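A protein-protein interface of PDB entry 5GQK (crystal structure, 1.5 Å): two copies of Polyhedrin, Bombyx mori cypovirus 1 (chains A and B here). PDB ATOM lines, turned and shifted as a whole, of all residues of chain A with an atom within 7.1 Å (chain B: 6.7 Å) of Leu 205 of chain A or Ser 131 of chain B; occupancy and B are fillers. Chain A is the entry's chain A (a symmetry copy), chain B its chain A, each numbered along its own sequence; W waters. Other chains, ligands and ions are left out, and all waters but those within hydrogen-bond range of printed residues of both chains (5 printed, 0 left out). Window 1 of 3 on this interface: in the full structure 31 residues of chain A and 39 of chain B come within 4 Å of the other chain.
Water W4 lies within hydrogen-bond range of OD1 of Asn 52 of chain A, O of Val 130 of chain B and OH of Tyr 227 of chain A.
Water W1 lies within hydrogen-bond range of O of Leu 203 of chain A (2.7 Å) and O of Pro 142 of chain B (2.8 Å).
Water W3 lies within hydrogen-bond range of the side-chain hydroxyl (OG) of Ser 62 of chain B, the backbone NH (N) of Arg 206 of chain A and the backbone carbonyl oxygen (O) of Glu 63 of chain B.
Water W2 lies within hydrogen-bond range of the side-chain hydroxyl (OG1) of Thr 64 of chain B (2.7 Å) and the side-chain sulfur (SG) of Cys 208 of chain A (3.7 Å).
Water W5 lies within hydrogen-bond range of O of Leu 137 of chain B and N of Glu 34 of chain A.
Of the 16 printed residues of chain A, 9 touch a printed residue of chain B.
Hydrophobic or aromatic side chains of chain A that line the printed part of chain B: Leu 203, Leu 205, Phe 207 and Tyr 227.
Hydrophobic or aromatic side chains of chain B that line the printed part of chain A: Ala 125, Val 130, Val 132, Pro 133, Leu 137, Pro 142 and Ala 178.
OG of Ser 62 of chain B lies within hydrogen-bond range of O of Ala 204 of chain A (2.7 Å).
O of Ser 131 of chain B sits at hydrogen-bond distance from ND2 of Asn 54 of chain A, at 2.9 Å.
O of Arg 206 of chain A lies within hydrogen-bond range of OG of Ser 131 of chain B, at 2.7 Å.
Of chain B, only Ala 125 (3.7 Å), Ser 131 (3.7 Å), Pro 133 (3.9 Å), Leu 177 (3.9 Å) and Ala 178 (3.7 Å) come within 4 Å of Leu 205 of chain A.
Of the printed residues of chain B, Arg 206 of chain A touches Thr 64 (3.2 Å) and Ser 131 (2.7 Å).
Of chain A, only Asn 54, Leu 205, Arg 206 and Phe 207 come within 4 Å of Ser 131 of chain B.
Of the printed residues of chain A, Ala 178 of chain B touches Asp 202, Leu 203 and Leu 205.
The nearest residue of chain B that does not touch Leu 205 of chain A is Gly 127 of chain B (4.1 Å).
OD1 of Asn 128 of chain B sits at hydrogen-bond distance from N of Ser 131 of chain B.
N of Val 132 of chain B is in hydrogen-bond range of OD1 of Asn 128 of chain B, at 3.1 Å.
The backbone NH (N) of Ser 55 of chain A is in hydrogen-bond range of the side-chain carboxylate (OE1) of Glu 34 of chain A.
O of Phe 207 of chain A sits at hydrogen-bond distance from N of Asn 52 of chain A (2.8 Å).
N of Leu 205 of chain A is in hydrogen-bond range of O of Asn 54 of chain A (3.0 Å).
SG of Cys 208 of chain A lies within hydrogen-bond range of NH1 of Arg 206 of chain A, 3.4 Å away.
No position is printed for both chains.
Of the 22 pairs that touch across the chains among the printed residues, none has its exchanged pair printed and touching as well.
Pro 133 of chain B touches Glu 34 of chain A.
CG of Glu 34 of chain A touches O of Leu 137 of chain B, 3.7 Å away.
CD2 of Leu 137 of chain B touches CG of Asn 54 of chain A, at 3.5 Å.
Leu 203 of chain A touches Ala 125 of chain B (O to CB, 3.8 Å).
CD1 of Leu 205 of chain A touches CG of Pro 133 of chain B, 3.9 Å away.
CD2 of Leu 205 of chain A touches N of Ala 178 of chain B, 3.7 Å away.
CD1 of Phe 207 of chain A touches O of Ala 129 of chain B, at 3.8 Å.
Phe 207 of chain A touches Val 130 of chain B.
OG of Ser 131 of chain B touches CB of Phe 207 of chain A (3.5 Å).
Leu 137 of chain B touches Tyr 227 of chain A.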
ATOM      1  N   GLU A  34       3.580  33.434  -0.986  1.00  0.00           N
ATOM      2  CA  GLU A  34       2.228  33.916  -1.043  1.00  0.00           C
ATOM      3  C   GLU A  34       2.162  35.417  -1.110  1.00  0.00           C
ATOM      4  O   GLU A  34       3.021  36.148  -0.546  1.00  0.00           O
ATOM      5  CB  GLU A  34       1.515  33.521   0.250  1.00  0.00           C
ATOM      6  CG  GLU A  34       1.190  32.015   0.402  1.00  0.00           C
ATOM      7  CD  GLU A  34      -0.024  31.603  -0.376  1.00  0.00           C
ATOM      8  OE1 GLU A  34      -0.605  32.358  -1.197  1.00  0.00           O
ATOM      9  OE2 GLU A  34      -0.341  30.416  -0.305  1.00  0.00           O
ATOM     10  N   ASN A  52     -10.904  36.509   2.475  1.00  0.00           N
ATOM     11  CA  ASN A  52      -9.452  36.455   2.298  1.00  0.00           C
ATOM     12  C   ASN A  52      -9.151  35.670   1.009  1.00  0.00           C
ATOM     13  O   ASN A  52      -9.783  34.621   0.734  1.00  0.00           O
ATOM     14  CB  ASN A  52      -8.863  35.728   3.519  1.00  0.00           C
ATOM     15  CG  ASN A  52      -7.390  35.330   3.409  1.00  0.00           C
ATOM     16  OD1 ASN A  52      -7.078  34.256   3.871  1.00  0.00           O
ATOM     17  ND2 ASN A  52      -6.490  36.166   2.861  1.00  0.00           N
ATOM     18  N   LYS A  53      -8.166  36.156   0.249  1.00  0.00           N
ATOM     19  CA  LYS A  53      -7.604  35.362  -0.877  1.00  0.00           C
ATOM     20  C   LYS A  53      -6.092  35.306  -0.702  1.00  0.00           C
ATOM     21  O   LYS A  53      -5.437  36.335  -0.427  1.00  0.00           O
ATOM     22  CB  LYS A  53      -7.944  36.062  -2.212  1.00  0.00           C
ATOM     23  CG  LYS A  53      -7.763  35.163  -3.393  1.00  0.00           C
ATOM     24  CD  LYS A  53      -9.077  34.351  -3.621  1.00  0.00           C
ATOM     25  CE  LYS A  53     -10.152  35.169  -4.369  1.00  0.00           C
ATOM     26  NZ  LYS A  53      -9.922  35.490  -5.819  1.00  0.00           N
ATOM     27  N   ASN A  54      -5.528  34.108  -0.932  1.00  0.00           N
ATOM     28  CA  ASN A  54      -4.098  33.891  -0.769  1.00  0.00           C
ATOM     29  C   ASN A  54      -3.640  33.221  -2.055  1.00  0.00           C
ATOM     30  O   ASN A  54      -4.165  32.168  -2.415  1.00  0.00           O
ATOM     31  CB  ASN A  54      -3.884  32.872   0.353  1.00  0.00           C
ATOM     32  CG  ASN A  54      -4.426  33.373   1.705  1.00  0.00           C
ATOM     33  OD1 ASN A  54      -4.161  34.514   2.083  1.00  0.00           O
ATOM     34  ND2 ASN A  54      -5.196  32.572   2.397  1.00  0.00           N
ATOM     35  N   SER A  55      -2.696  33.808  -2.761  1.00  0.00           N
ATOM     36  CA  SER A  55      -2.236  33.191  -3.996  1.00  0.00           C
ATOM     37  C   SER A  55      -0.808  33.618  -4.285  1.00  0.00           C
ATOM     38  O   SER A  55      -0.323  34.661  -3.798  1.00  0.00           O
ATOM     39  CB  SER A  55      -3.101  33.705  -5.165  1.00  0.00           C
ATOM     40  OG  SER A  55      -3.021  32.842  -6.337  1.00  0.00           O
ATOM     41  N   VAL A  59      -2.920  38.672  -6.376  1.00  0.00           N
ATOM     42  CA  VAL A  59      -4.130  38.226  -5.731  1.00  0.00           C
ATOM     43  C   VAL A  59      -5.181  39.339  -5.708  1.00  0.00           C
ATOM     44  O   VAL A  59      -4.834  40.504  -5.784  1.00  0.00           O
ATOM     45  CB  VAL A  59      -3.744  37.818  -4.288  1.00  0.00           C
ATOM     46  CG1 VAL A  59      -3.460  39.018  -3.394  1.00  0.00           C
ATOM     47  CG2 VAL A  59      -4.838  36.916  -3.697  1.00  0.00           C
ATOM     48  N   SER A 200      -1.873  30.008 -11.141  1.00  0.00           N
ATOM     49  CA  SER A 200      -2.110  30.651  -9.851  1.00  0.00           C
ATOM     50  C   SER A 200      -3.536  31.208  -9.726  1.00  0.00           C
ATOM     51  O   SER A 200      -4.058  31.213  -8.634  1.00  0.00           O
ATOM     52  CB  SER A 200      -1.039  31.739  -9.602  1.00  0.00           C
ATOM     53  OG  SER A 200      -1.413  32.996 -10.206  1.00  0.00           O
ATOM     54  N   CYS A 201      -4.157  31.586 -10.857  1.00  0.00           N
ATOM     55  CA  CYS A 201      -5.566  32.056 -10.840  1.00  0.00           C
ATOM     56  C   CYS A 201      -6.465  30.894 -10.380  1.00  0.00           C
ATOM     57  O   CYS A 201      -7.427  31.167  -9.710  1.00  0.00           O
ATOM     58  CB  CYS A 201      -5.984  32.486 -12.237  1.00  0.00           C
ATOM     59  SG  CYS A 201      -5.115  33.971 -12.790  1.00  0.00           S
ATOM     60  N   ASP A 202      -6.162  29.633 -10.714  1.00  0.00           N
ATOM     61  CA  ASP A 202      -6.982  28.544 -10.275  1.00  0.00           C
ATOM     62  C   ASP A 202      -6.608  28.092  -8.869  1.00  0.00           C
ATOM     63  O   ASP A 202      -7.465  27.545  -8.165  1.00  0.00           O
ATOM     64  CB  ASP A 202      -6.855  27.388 -11.234  1.00  0.00           C
ATOM     65  CG  ASP A 202      -7.664  27.622 -12.487  1.00  0.00           C
ATOM     66  OD1 ASP A 202      -8.887  27.862 -12.378  1.00  0.00           O
ATOM     67  OD2 ASP A 202      -7.082  27.588 -13.562  1.00  0.00           O
ATOM     68  N   LEU A 203      -5.342  28.273  -8.509  1.00  0.00           N
ATOM     69  CA  LEU A 203      -4.802  27.767  -7.256  1.00  0.00           C
ATOM     70  C   LEU A 203      -5.059  28.660  -6.025  1.00  0.00           C
ATOM     71  O   LEU A 203      -4.907  28.205  -4.847  1.00  0.00           O
ATOM     72  CB  LEU A 203      -3.298  27.467  -7.386  1.00  0.00           C
ATOM     73  CG  LEU A 203      -3.019  26.259  -8.304  1.00  0.00           C
ATOM     74  CD1 LEU A 203      -1.569  26.276  -8.828  1.00  0.00           C
ATOM     75  CD2 LEU A 203      -3.376  24.935  -7.583  1.00  0.00           C
ATOM     76  N   ALA A 204      -5.444  29.896  -6.309  1.00  0.00           N
ATOM     77  CA  ALA A 204      -5.696  30.883  -5.238  1.00  0.00           C
ATOM     78  C   ALA A 204      -6.716  30.287  -4.284  1.00  0.00           C
ATOM     79  O   ALA A 204      -7.766  29.809  -4.721  1.00  0.00           O
ATOM     80  CB  ALA A 204      -6.220  32.180  -5.816  1.00  0.00           C
ATOM     81  N   LEU A 205      -6.435  30.341  -2.984  1.00  0.00           N
ATOM     82  CA  LEU A 205      -7.411  29.833  -2.010  1.00  0.00           C
ATOM     83  C   LEU A 205      -8.220  30.961  -1.412  1.00  0.00           C
ATOM     84  O   LEU A 205      -7.666  32.055  -1.178  1.00  0.00           O
ATOM     85  CB  LEU A 205      -6.634  29.105  -0.920  1.00  0.00           C
ATOM     86  CG  LEU A 205      -6.055  27.717  -1.276  1.00  0.00           C
ATOM     87  CD1 LEU A 205      -5.271  27.210  -0.090  1.00  0.00           C
ATOM     88  CD2 LEU A 205      -7.138  26.684  -1.654  1.00  0.00           C
ATOM     89  N   ARG A 206      -9.501  30.723  -1.220  1.00  0.00           N
ATOM     90  CA  ARG A 206     -10.418  31.743  -0.729  1.00  0.00           C
ATOM     91  C   ARG A 206     -10.949  31.332   0.612  1.00  0.00           C
ATOM     92  O   ARG A 206     -11.144  30.121   0.895  1.00  0.00           O
ATOM     93  CB  ARG A 206     -11.593  31.945  -1.702  1.00  0.00           C
ATOM     94  CG  ARG A 206     -12.573  33.114  -1.297  1.00  0.00           C
ATOM     95  CD  ARG A 206     -13.530  33.425  -2.462  1.00  0.00           C
ATOM     96  NE  ARG A 206     -14.489  34.519  -2.140  1.00  0.00           N
ATOM     97  CZ  ARG A 206     -15.633  34.312  -1.486  1.00  0.00           C
ATOM     98  NH1 ARG A 206     -15.897  33.083  -1.074  1.00  0.00           N
ATOM     99  NH2 ARG A 206     -16.475  35.316  -1.191  1.00  0.00           N
ATOM    100  N   PHE A 207     -11.224  32.316   1.470  1.00  0.00           N
ATOM    101  CA  PHE A 207     -11.901  32.000   2.783  1.00  0.00           C
ATOM    102  C   PHE A 207     -12.907  33.123   3.020  1.00  0.00           C
ATOM    103  O   PHE A 207     -12.599  34.321   2.786  1.00  0.00           O
ATOM    104  CB  PHE A 207     -10.879  31.990   3.877  1.00  0.00           C
ATOM    105  CG  PHE A 207     -11.455  31.925   5.282  1.00  0.00           C
ATOM    106  CD1 PHE A 207     -11.841  30.658   5.839  1.00  0.00           C
ATOM    107  CD2 PHE A 207     -11.673  33.138   6.017  1.00  0.00           C
ATOM    108  CE1 PHE A 207     -12.399  30.611   7.127  1.00  0.00           C
ATOM    109  CE2 PHE A 207     -12.218  33.071   7.317  1.00  0.00           C
ATOM    110  CZ  PHE A 207     -12.572  31.798   7.850  1.00  0.00           C
ATOM    111  N   CYS A 208     -14.087  32.789   3.525  1.00  0.00           N
ATOM    112  CA  CYS A 208     -14.989  33.842   3.978  1.00  0.00           C
ATOM    113  C   CYS A 208     -15.814  33.389   5.127  1.00  0.00           C
ATOM    114  O   CYS A 208     -16.218  32.242   5.215  1.00  0.00           O
ATOM    115  CB  CYS A 208     -15.866  34.397   2.876  1.00  0.00           C
ATOM    116  SG  CYS A 208     -17.005  33.223   2.142  1.00  0.00           S
ATOM    117  N   TYR A 227      -1.824  36.691  11.193  1.00  0.00           N
ATOM    118  CA  TYR A 227      -2.181  37.693  10.218  1.00  0.00           C
ATOM    119  C   TYR A 227      -2.009  39.106  10.805  1.00  0.00           C
ATOM    120  O   TYR A 227      -2.070  39.308  12.032  1.00  0.00           O
ATOM    121  CB  TYR A 227      -3.670  37.559   9.866  1.00  0.00           C
ATOM    122  CG  TYR A 227      -4.021  36.296   9.097  1.00  0.00           C
ATOM    123  CD1 TYR A 227      -3.038  35.471   8.479  1.00  0.00           C
ATOM    124  CD2 TYR A 227      -5.354  35.961   8.974  1.00  0.00           C
ATOM    125  CE1 TYR A 227      -3.401  34.325   7.780  1.00  0.00           C
ATOM    126  CE2 TYR A 227      -5.742  34.804   8.300  1.00  0.00           C
ATOM    127  CZ  TYR A 227      -4.772  34.002   7.707  1.00  0.00           C
ATOM    128  OH  TYR A 227      -5.171  32.877   7.034  1.00  0.00           O
ATOM    129  N   SER B  62     -11.356  25.729  -7.320  1.00  0.00           N
ATOM    130  CA  SER B  62     -10.878  26.197  -6.017  1.00  0.00           C
ATOM    131  C   SER B  62     -12.089  26.372  -5.131  1.00  0.00           C
ATOM    132  O   SER B  62     -12.993  27.140  -5.483  1.00  0.00           O
ATOM    133  CB  SER B  62     -10.062  27.533  -6.131  1.00  0.00           C
ATOM    134  OG  SER B  62      -9.785  27.945  -4.787  1.00  0.00           O
ATOM    135  N   GLU B  63     -12.108  25.651  -4.022  1.00  0.00           N
ATOM    136  CA  GLU B  63     -13.226  25.716  -3.111  1.00  0.00           C
ATOM    137  C   GLU B  63     -12.789  25.993  -1.663  1.00  0.00           C
ATOM    138  O   GLU B  63     -11.739  25.527  -1.241  1.00  0.00           O
ATOM    139  CB  GLU B  63     -14.081  24.440  -3.191  1.00  0.00           C
ATOM    140  CG  GLU B  63     -14.615  24.170  -4.622  1.00  0.00           C
ATOM    141  CD  GLU B  63     -15.680  25.203  -5.071  1.00  0.00           C
ATOM    142  OE1 GLU B  63     -16.368  25.844  -4.220  1.00  0.00           O
ATOM    143  OE2 GLU B  63     -15.867  25.361  -6.319  1.00  0.00           O
ATOM    144  N   THR B  64     -13.665  26.655  -0.899  1.00  0.00           N
ATOM    145  CA  THR B  64     -13.449  26.865   0.538  1.00  0.00           C
ATOM    146  C   THR B  64     -13.778  25.578   1.307  1.00  0.00           C
ATOM    147  O   THR B  64     -14.434  24.665   0.762  1.00  0.00           O
ATOM    148  CB  THR B  64     -14.400  27.962   1.112  1.00  0.00           C
ATOM    149  OG1 THR B  64     -15.766  27.533   1.035  1.00  0.00           O
ATOM    150  CG2 THR B  64     -14.221  29.302   0.416  1.00  0.00           C
ATOM    151  N   PHE B  65     -13.350  25.508   2.572  1.00  0.00           N
ATOM    152  CA  PHE B  65     -13.800  24.431   3.453  1.00  0.00           C
ATOM    153  C   PHE B  65     -15.333  24.324   3.477  1.00  0.00           C
ATOM    154  O   PHE B  65     -15.941  23.213   3.334  1.00  0.00           O
ATOM    155  CB  PHE B  65     -13.230  24.626   4.871  1.00  0.00           C
ATOM    156  CG  PHE B  65     -13.907  23.729   5.898  1.00  0.00           C
ATOM    157  CD1 PHE B  65     -13.532  22.367   6.027  1.00  0.00           C
ATOM    158  CD2 PHE B  65     -14.954  24.239   6.702  1.00  0.00           C
ATOM    159  CE1 PHE B  65     -14.219  21.548   6.907  1.00  0.00           C
ATOM    160  CE2 PHE B  65     -15.630  23.385   7.625  1.00  0.00           C
ATOM    161  CZ  PHE B  65     -15.225  22.039   7.730  1.00  0.00           C
ATOM    162  N   ALA B 125      -3.338  22.877  -4.175  1.00  0.00           N
ATOM    163  CA  ALA B 125      -3.231  23.622  -2.919  1.00  0.00           C
ATOM    164  C   ALA B 125      -4.252  23.019  -1.959  1.00  0.00           C
ATOM    165  O   ALA B 125      -5.465  23.348  -1.995  1.00  0.00           O
ATOM    166  CB  ALA B 125      -3.487  25.135  -3.129  1.00  0.00           C
ATOM    167  N   LYS B 126      -3.780  22.133  -1.085  1.00  0.00           N
ATOM    168  CA  LYS B 126      -4.705  21.538  -0.107  1.00  0.00           C
ATOM    169  C   LYS B 126      -4.459  22.327   1.138  1.00  0.00           C
ATOM    170  O   LYS B 126      -3.403  22.175   1.807  1.00  0.00           O
ATOM    171  CB  LYS B 126      -4.356  20.051   0.058  1.00  0.00           C
ATOM    172  CG  LYS B 126      -5.167  19.359   1.171  1.00  0.00           C
ATOM    173  CD  LYS B 126      -5.101  17.833   1.062  1.00  0.00           C
ATOM    174  CE  LYS B 126      -3.758  17.265   1.488  1.00  0.00           C
ATOM    175  NZ  LYS B 126      -3.368  17.523   2.908  1.00  0.00           N
ATOM    176  N   GLY B 127      -5.393  23.220   1.422  1.00  0.00           N
ATOM    177  CA  GLY B 127      -5.267  24.115   2.563  1.00  0.00           C
ATOM    178  C   GLY B 127      -5.888  23.552   3.831  1.00  0.00           C
ATOM    179  O   GLY B 127      -6.587  22.502   3.802  1.00  0.00           O
ATOM    180  N   ASN B 128      -5.591  24.229   4.940  1.00  0.00           N
ATOM    181  CA  ASN B 128      -6.311  23.929   6.149  1.00  0.00           C
ATOM    182  C   ASN B 128      -7.685  24.595   6.116  1.00  0.00           C
ATOM    183  O   ASN B 128      -8.104  25.129   5.071  1.00  0.00           O
ATOM    184  CB  ASN B 128      -5.504  24.312   7.365  1.00  0.00           C
ATOM    185  CG  ASN B 128      -5.321  25.830   7.516  1.00  0.00           C
ATOM    186  OD1 ASN B 128      -5.934  26.650   6.822  1.00  0.00           O
ATOM    187  ND2 ASN B 128      -4.490  26.202   8.446  1.00  0.00           N
ATOM    188  N   ALA B 129      -8.423  24.552   7.219  1.00  0.00           N
ATOM    189  CA  ALA B 129      -9.812  25.041   7.177  1.00  0.00           C
ATOM    190  C   ALA B 129      -9.945  26.552   6.991  1.00  0.00           C
ATOM    191  O   ALA B 129     -11.017  27.015   6.587  1.00  0.00           O
ATOM    192  CB  ALA B 129     -10.623  24.575   8.380  1.00  0.00           C
ATOM    193  N   VAL B 130      -8.857  27.298   7.167  1.00  0.00           N
ATOM    194  CA  VAL B 130      -8.899  28.743   6.946  1.00  0.00           C
ATOM    195  C   VAL B 130      -8.164  29.124   5.678  1.00  0.00           C
ATOM    196  O   VAL B 130      -7.813  30.269   5.477  1.00  0.00           O
ATOM    197  CB  VAL B 130      -8.434  29.562   8.186  1.00  0.00           C
ATOM    198  CG1 VAL B 130      -9.422  29.326   9.301  1.00  0.00           C
ATOM    199  CG2 VAL B 130      -7.013  29.162   8.655  1.00  0.00           C
ATOM    200  N   SER B 131      -7.846  28.117   4.834  1.00  0.00           N
ATOM    201  CA  SER B 131      -7.415  28.391   3.429  1.00  0.00           C
ATOM    202  C   SER B 131      -5.958  28.805   3.394  1.00  0.00           C
ATOM    203  O   SER B 131      -5.554  29.677   2.599  1.00  0.00           O
ATOM    204  CB  SER B 131      -8.269  29.436   2.739  1.00  0.00           C
ATOM    205  OG  SER B 131      -9.604  28.894   2.717  1.00  0.00           O
ATOM    206  N   VAL B 132      -5.172  28.174   4.276  1.00  0.00           N
ATOM    207  CA  VAL B 132      -3.715  28.364   4.318  1.00  0.00           C
ATOM    208  C   VAL B 132      -3.023  27.056   3.853  1.00  0.00           C
ATOM    209  O   VAL B 132      -3.306  26.002   4.411  1.00  0.00           O
ATOM    210  CB  VAL B 132      -3.245  28.807   5.739  1.00  0.00           C
ATOM    211  CG1 VAL B 132      -1.715  28.855   5.848  1.00  0.00           C
ATOM    212  CG2 VAL B 132      -3.835  30.177   6.029  1.00  0.00           C
ATOM    213  N   PRO B 133      -2.110  27.116   2.820  1.00  0.00           N
ATOM    214  CA  PRO B 133      -1.567  25.827   2.310  1.00  0.00           C
ATOM    215  C   PRO B 133      -0.773  25.025   3.288  1.00  0.00           C
ATOM    216  O   PRO B 133      -0.870  23.786   3.253  1.00  0.00           O
ATOM    217  CB  PRO B 133      -0.697  26.265   1.116  1.00  0.00           C
ATOM    218  CG  PRO B 133      -1.444  27.466   0.588  1.00  0.00           C
ATOM    219  CD  PRO B 133      -1.752  28.211   1.880  1.00  0.00           C
ATOM    220  N   LEU B 137       0.858  31.401   6.319  1.00  0.00           N
ATOM    221  CA  LEU B 137       1.091  31.905   4.963  1.00  0.00           C
ATOM    222  C   LEU B 137       2.571  32.173   4.725  1.00  0.00           C
ATOM    223  O   LEU B 137       3.091  31.930   3.616  1.00  0.00           O
ATOM    224  CB  LEU B 137       0.360  33.226   4.774  1.00  0.00           C
ATOM    225  CG  LEU B 137      -1.173  33.070   4.679  1.00  0.00           C
ATOM    226  CD1 LEU B 137      -1.875  34.439   4.703  1.00  0.00           C
ATOM    227  CD2 LEU B 137      -1.612  32.272   3.407  1.00  0.00           C
ATOM    228  N   PRO B 142       2.648  27.981  -2.409  1.00  0.00           N
ATOM    229  CA  PRO B 142       1.193  27.978  -2.645  1.00  0.00           C
ATOM    230  C   PRO B 142       0.640  26.721  -3.329  1.00  0.00           C
ATOM    231  O   PRO B 142      -0.547  26.670  -3.601  1.00  0.00           O
ATOM    232  CB  PRO B 142       0.965  29.241  -3.505  1.00  0.00           C
ATOM    233  CG  PRO B 142       2.121  30.150  -3.105  1.00  0.00           C
ATOM    234  CD  PRO B 142       3.277  29.156  -3.073  1.00  0.00           C
ATOM    235  N   ILE B 175     -10.293  20.417   5.347  1.00  0.00           N
ATOM    236  CA  ILE B 175      -9.495  21.054   4.254  1.00  0.00           C
ATOM    237  C   ILE B 175     -10.253  22.086   3.426  1.00  0.00           C
ATOM    238  O   ILE B 175     -11.502  22.050   3.298  1.00  0.00           O
ATOM    239  CB  ILE B 175      -8.868  20.026   3.288  1.00  0.00           C
ATOM    240  CG1 ILE B 175      -9.961  19.358   2.443  1.00  0.00           C
ATOM    241  CG2 ILE B 175      -7.977  19.015   4.034  1.00  0.00           C
ATOM    242  CD1 ILE B 175      -9.414  18.549   1.240  1.00  0.00           C
ATOM    243  N   SER B 176      -9.449  22.992   2.846  1.00  0.00           N
ATOM    244  CA  SER B 176      -9.850  23.803   1.689  1.00  0.00           C
ATOM    245  C   SER B 176      -9.054  23.252   0.511  1.00  0.00           C
ATOM    246  O   SER B 176      -8.121  22.535   0.714  1.00  0.00           O
ATOM    247  CB  SER B 176      -9.545  25.278   1.964  1.00  0.00           C
ATOM    248  OG  SER B 176      -8.145  25.404   2.297  1.00  0.00           O
ATOM    249  N   LEU B 177      -9.442  23.528  -0.715  1.00  0.00           N
ATOM    250  CA  LEU B 177      -8.835  22.761  -1.838  1.00  0.00           C
ATOM    251  C   LEU B 177      -8.862  23.528  -3.148  1.00  0.00           C
ATOM    252  O   LEU B 177      -9.938  23.935  -3.581  1.00  0.00           O
ATOM    253  CB  LEU B 177      -9.588  21.397  -2.003  1.00  0.00           C
ATOM    254  CG  LEU B 177      -8.943  20.491  -3.085  1.00  0.00           C
ATOM    255  CD1 LEU B 177      -7.518  20.086  -2.666  1.00  0.00           C
ATOM    256  CD2 LEU B 177      -9.865  19.281  -3.283  1.00  0.00           C
ATOM    257  N   ALA B 178      -7.697  23.657  -3.791  1.00  0.00           N
ATOM    258  CA  ALA B 178      -7.674  24.039  -5.189  1.00  0.00           C
ATOM    259  C   ALA B 178      -6.773  23.133  -5.966  1.00  0.00           C
ATOM    260  O   ALA B 178      -5.773  22.594  -5.425  1.00  0.00           O
ATOM    261  CB  ALA B 178      -7.150  25.489  -5.351  1.00  0.00           C
HETATM  262  O   HOH W   1      -2.447  28.743  -3.921  1.00  0.00           O
HETATM  263  O   HOH W   2     -17.480  29.667   1.284  1.00  0.00           O
HETATM  264  O   HOH W   3     -10.616  28.198  -2.205  1.00  0.00           O
HETATM  265  O   HOH W   4      -7.818  32.934   6.066  1.00  0.00           O
HETATM  266  O   HOH W   5       4.724  32.192   1.388  1.00  0.00           O
